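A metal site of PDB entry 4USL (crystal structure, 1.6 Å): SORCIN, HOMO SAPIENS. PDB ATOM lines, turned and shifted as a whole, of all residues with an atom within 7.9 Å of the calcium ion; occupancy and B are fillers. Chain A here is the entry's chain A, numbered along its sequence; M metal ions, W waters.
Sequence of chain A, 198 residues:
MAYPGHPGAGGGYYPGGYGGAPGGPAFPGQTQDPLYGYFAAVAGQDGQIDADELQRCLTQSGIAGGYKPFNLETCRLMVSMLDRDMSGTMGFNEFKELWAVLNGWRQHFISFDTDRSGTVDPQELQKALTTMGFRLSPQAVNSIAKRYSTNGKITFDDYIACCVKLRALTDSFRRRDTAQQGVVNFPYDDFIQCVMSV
The side-chain hydroxyl of Thr 89 sits at hydrogen-bond distance from the side-chain amide nitrogen of Gln 48 (2.8 Å). The side-chain carboxylate (OD2) of Asp 83 lies within hydrogen-bond range of the backbone NH (N) of Gly 88 (2.8 Å). OE2 of Glu 94 lies close to N of Arg 84, 2.9 Å away. N of Gly 91 lies close to OE1 of Glu 94, at 3.1 Å.
Within 4 Å of the calcium ion: Asp 83, Asp 85, Ser 87, Thr 89 and Glu 94.
The calcium ion is bound by the side-chain carboxylate (OD1) of Asp 83, water W1, the side-chain carboxylate (OD1) of Asp 85, the backbone carbonyl oxygen (O) of Thr 89, the side-chain carboxylate (OE1) of Glu 94, the side-chain hydroxyl (OG) of Ser 87 and the side-chain carboxylate (OE2) of Glu 94.
Water W1 lies within hydrogen-bond range of the side-chain amide nitrogen (NE2) of Gln 48 (2.8 Å), the backbone NH (N) of Gly 91 (3.2 Å) and the side-chain carboxylate (OD2) of Asp 85 (3.3 Å).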
ATOM      1  N   GLN A  48      -2.466 -33.646  26.255  1.00  0.00           N
ATOM      2  CA  GLN A  48      -1.065 -33.203  26.407  1.00  0.00           C
ATOM      3  C   GLN A  48      -0.203 -33.966  25.424  1.00  0.00           C
ATOM      4  O   GLN A  48      -0.490 -35.122  25.076  1.00  0.00           O
ATOM      5  CB  GLN A  48      -0.554 -33.476  27.828  1.00  0.00           C
ATOM      6  CG  GLN A  48      -1.264 -32.676  28.926  1.00  0.00           C
ATOM      7  CD  GLN A  48      -0.953 -31.174  28.898  1.00  0.00           C
ATOM      8  OE1 GLN A  48      -1.885 -30.337  28.892  1.00  0.00           O
ATOM      9  NE2 GLN A  48       0.328 -30.806  28.878  1.00  0.00           N
ATOM     10  N   ILE A  49       0.898 -33.331  25.027  1.00  0.00           N
ATOM     11  CA  ILE A  49       1.834 -33.970  24.091  1.00  0.00           C
ATOM     12  C   ILE A  49       2.999 -34.544  24.902  1.00  0.00           C
ATOM     13  O   ILE A  49       3.663 -33.819  25.635  1.00  0.00           O
ATOM     14  CB  ILE A  49       2.311 -32.987  22.999  1.00  0.00           C
ATOM     15  CG1 ILE A  49       1.134 -32.632  22.054  1.00  0.00           C
ATOM     16  CG2 ILE A  49       3.493 -33.559  22.191  1.00  0.00           C
ATOM     17  CD1 ILE A  49       1.387 -31.478  21.138  1.00  0.00           C
ATOM     18  N   VAL A  79      10.557 -30.803  24.984  1.00  0.00           N
ATOM     19  CA  VAL A  79       9.481 -30.947  25.972  1.00  0.00           C
ATOM     20  C   VAL A  79       9.978 -30.420  27.335  1.00  0.00           C
ATOM     21  O   VAL A  79       9.278 -29.668  28.023  1.00  0.00           O
ATOM     22  CB  VAL A  79       8.952 -32.394  26.122  1.00  0.00           C
ATOM     23  CG1 VAL A  79       7.959 -32.489  27.269  1.00  0.00           C
ATOM     24  CG2 VAL A  79       8.276 -32.853  24.852  1.00  0.00           C
ATOM     25  N   SER A  80      11.212 -30.790  27.679  1.00  0.00           N
ATOM     26  CA  SER A  80      11.763 -30.425  28.980  1.00  0.00           C
ATOM     27  C   SER A  80      12.037 -28.935  29.081  1.00  0.00           C
ATOM     28  O   SER A  80      11.685 -28.286  30.084  1.00  0.00           O
ATOM     29  CB  SER A  80      13.052 -31.211  29.249  1.00  0.00           C
ATOM     30  OG  SER A  80      12.753 -32.348  30.026  1.00  0.00           O
ATOM     31  N   LEU A  82      10.913 -26.339  27.189  1.00  0.00           N
ATOM     32  CA  LEU A  82       9.768 -25.457  27.013  1.00  0.00           C
ATOM     33  C   LEU A  82       8.719 -25.525  28.114  1.00  0.00           C
ATOM     34  O   LEU A  82       7.780 -24.723  28.146  1.00  0.00           O
ATOM     35  CB  LEU A  82       9.080 -25.788  25.680  1.00  0.00           C
ATOM     36  CG  LEU A  82       9.945 -25.472  24.463  1.00  0.00           C
ATOM     37  CD1 LEU A  82       9.351 -26.096  23.209  1.00  0.00           C
ATOM     38  CD2 LEU A  82      10.016 -23.978  24.230  1.00  0.00           C
ATOM     39  N   ASP A  83       8.886 -26.483  29.020  1.00  0.00           N
ATOM     40  CA  ASP A  83       7.893 -26.783  30.060  1.00  0.00           C
ATOM     41  C   ASP A  83       7.685 -25.540  30.953  1.00  0.00           C
ATOM     42  O   ASP A  83       8.661 -25.004  31.478  1.00  0.00           O
ATOM     43  CB  ASP A  83       8.356 -27.980  30.869  1.00  0.00           C
ATOM     44  CG  ASP A  83       7.213 -28.725  31.563  1.00  0.00           C
ATOM     45  OD1 ASP A  83       5.989 -28.446  31.324  1.00  0.00           O
ATOM     46  OD2 ASP A  83       7.553 -29.644  32.358  1.00  0.00           O
ATOM     47  N   ARG A  84       6.446 -25.103  31.091  1.00  0.00           N
ATOM     48  CA  ARG A  84       6.126 -23.907  31.880  1.00  0.00           C
ATOM     49  C   ARG A  84       5.540 -24.210  33.221  1.00  0.00           C
ATOM     50  O   ARG A  84       5.494 -23.312  34.064  1.00  0.00           O
ATOM     51  CB  ARG A  84       5.153 -22.960  31.147  1.00  0.00           C
ATOM     52  CG  ARG A  84       5.536 -22.608  29.744  1.00  0.00           C
ATOM     53  CD  ARG A  84       4.498 -21.765  29.019  1.00  0.00           C
ATOM     54  NE  ARG A  84       4.995 -21.325  27.729  1.00  0.00           N
ATOM     55  CZ  ARG A  84       4.548 -20.303  27.044  1.00  0.00           C
ATOM     56  NH1 ARG A  84       3.528 -19.560  27.487  1.00  0.00           N
ATOM     57  NH2 ARG A  84       5.127 -19.989  25.895  1.00  0.00           N
ATOM     58  N   ASP A  85       5.082 -25.447  33.423  1.00  0.00           N
ATOM     59  CA  ASP A  85       4.285 -25.792  34.589  1.00  0.00           C
ATOM     60  C   ASP A  85       4.801 -27.033  35.297  1.00  0.00           C
ATOM     61  O   ASP A  85       4.077 -27.639  36.081  1.00  0.00           O
ATOM     62  CB  ASP A  85       2.814 -25.976  34.207  1.00  0.00           C
ATOM     63  CG  ASP A  85       2.592 -27.000  33.094  1.00  0.00           C
ATOM     64  OD1 ASP A  85       3.576 -27.530  32.527  1.00  0.00           O
ATOM     65  OD2 ASP A  85       1.407 -27.262  32.783  1.00  0.00           O
ATOM     66  N   MET A  86       6.040 -27.412  35.000  1.00  0.00           N
ATOM     67  CA  MET A  86       6.644 -28.623  35.522  1.00  0.00           C
ATOM     68  C   MET A  86       5.770 -29.870  35.322  1.00  0.00           C
ATOM     69  O   MET A  86       5.808 -30.782  36.139  1.00  0.00           O
ATOM     70  CB  MET A  86       6.977 -28.433  37.011  1.00  0.00           C
ATOM     71  CG  MET A  86       8.035 -27.364  37.251  1.00  0.00           C
ATOM     72  SD  MET A  86       8.408 -27.147  39.009  1.00  0.00           S
ATOM     73  CE  MET A  86       6.926 -26.312  39.541  1.00  0.00           C
ATOM     74  N   SER A  87       4.984 -29.919  34.242  1.00  0.00           N
ATOM     75  CA  SER A  87       4.136 -31.088  33.980  1.00  0.00           C
ATOM     76  C   SER A  87       4.869 -32.235  33.287  1.00  0.00           C
ATOM     77  O   SER A  87       4.351 -33.343  33.281  1.00  0.00           O
ATOM     78  CB  SER A  87       2.914 -30.709  33.125  1.00  0.00           C
ATOM     79  OG  SER A  87       3.299 -30.594  31.758  1.00  0.00           O
ATOM     80  N   GLY A  88       6.033 -31.970  32.698  1.00  0.00           N
ATOM     81  CA  GLY A  88       6.805 -32.963  31.939  1.00  0.00           C
ATOM     82  C   GLY A  88       6.134 -33.419  30.634  1.00  0.00           C
ATOM     83  O   GLY A  88       6.511 -34.453  30.051  1.00  0.00           O
ATOM     84  N   THR A  89       5.155 -32.635  30.217  1.00  0.00           N
ATOM     85  CA  THR A  89       4.390 -32.855  28.992  1.00  0.00           C
ATOM     86  C   THR A  89       4.192 -31.502  28.367  1.00  0.00           C
ATOM     87  O   THR A  89       4.260 -30.482  29.046  1.00  0.00           O
ATOM     88  CB  THR A  89       2.995 -33.440  29.310  1.00  0.00           C
ATOM     89  OG1 THR A  89       2.226 -32.502  30.077  1.00  0.00           O
ATOM     90  CG2 THR A  89       3.141 -34.733  30.044  1.00  0.00           C
ATOM     91  N   MET A  90       3.863 -31.494  27.072  1.00  0.00           N
ATOM     92  CA  MET A  90       3.702 -30.272  26.314  1.00  0.00           C
ATOM     93  C   MET A  90       2.229 -29.880  26.070  1.00  0.00           C
ATOM     94  O   MET A  90       1.464 -30.626  25.399  1.00  0.00           O
ATOM     95  CB  MET A  90       4.458 -30.430  24.986  1.00  0.00           C
ATOM     96  CG  MET A  90       4.194 -29.369  23.935  1.00  0.00           C
ATOM     97  SD  MET A  90       5.326 -29.488  22.523  1.00  0.00           S
ATOM     98  CE  MET A  90       6.826 -28.848  23.202  1.00  0.00           C
ATOM     99  N   GLY A  91       1.818 -28.736  26.576  1.00  0.00           N
ATOM    100  CA  GLY A  91       0.482 -28.212  26.329  1.00  0.00           C
ATOM    101  C   GLY A  91       0.409 -27.268  25.165  1.00  0.00           C
ATOM    102  O   GLY A  91       1.380 -27.092  24.424  1.00  0.00           O
ATOM    103  N   PHE A  92      -0.747 -26.654  24.953  1.00  0.00           N
ATOM    104  CA  PHE A  92      -0.927 -25.897  23.746  1.00  0.00           C
ATOM    105  C   PHE A  92       0.013 -24.672  23.632  1.00  0.00           C
ATOM    106  O   PHE A  92       0.559 -24.414  22.598  1.00  0.00           O
ATOM    107  CB  PHE A  92      -2.376 -25.462  23.561  1.00  0.00           C
ATOM    108  CG  PHE A  92      -2.594 -24.639  22.360  1.00  0.00           C
ATOM    109  CD1 PHE A  92      -2.347 -25.172  21.094  1.00  0.00           C
ATOM    110  CD2 PHE A  92      -3.031 -23.339  22.453  1.00  0.00           C
ATOM    111  CE1 PHE A  92      -2.529 -24.426  19.968  1.00  0.00           C
ATOM    112  CE2 PHE A  92      -3.226 -22.584  21.320  1.00  0.00           C
ATOM    113  CZ  PHE A  92      -2.989 -23.130  20.070  1.00  0.00           C
ATOM    114  N   GLU A  94       2.901 -24.208  25.014  1.00  0.00           N
ATOM    115  CA  GLU A  94       4.239 -24.784  24.861  1.00  0.00           C
ATOM    116  C   GLU A  94       4.460 -25.282  23.414  1.00  0.00           C
ATOM    117  O   GLU A  94       5.546 -25.112  22.844  1.00  0.00           O
ATOM    118  CB  GLU A  94       4.490 -25.883  25.885  1.00  0.00           C
ATOM    119  CG  GLU A  94       4.587 -25.359  27.309  1.00  0.00           C
ATOM    120  CD  GLU A  94       4.338 -26.386  28.379  1.00  0.00           C
ATOM    121  OE1 GLU A  94       4.311 -27.617  28.082  1.00  0.00           O
ATOM    122  OE2 GLU A  94       4.155 -26.002  29.567  1.00  0.00           O
HETATM  123 CA    CA M   1       3.851 -28.495  30.390  1.00  0.00          CA
HETATM  124  O   HOH W   1       1.579 -28.503  29.752  1.00  0.00           O
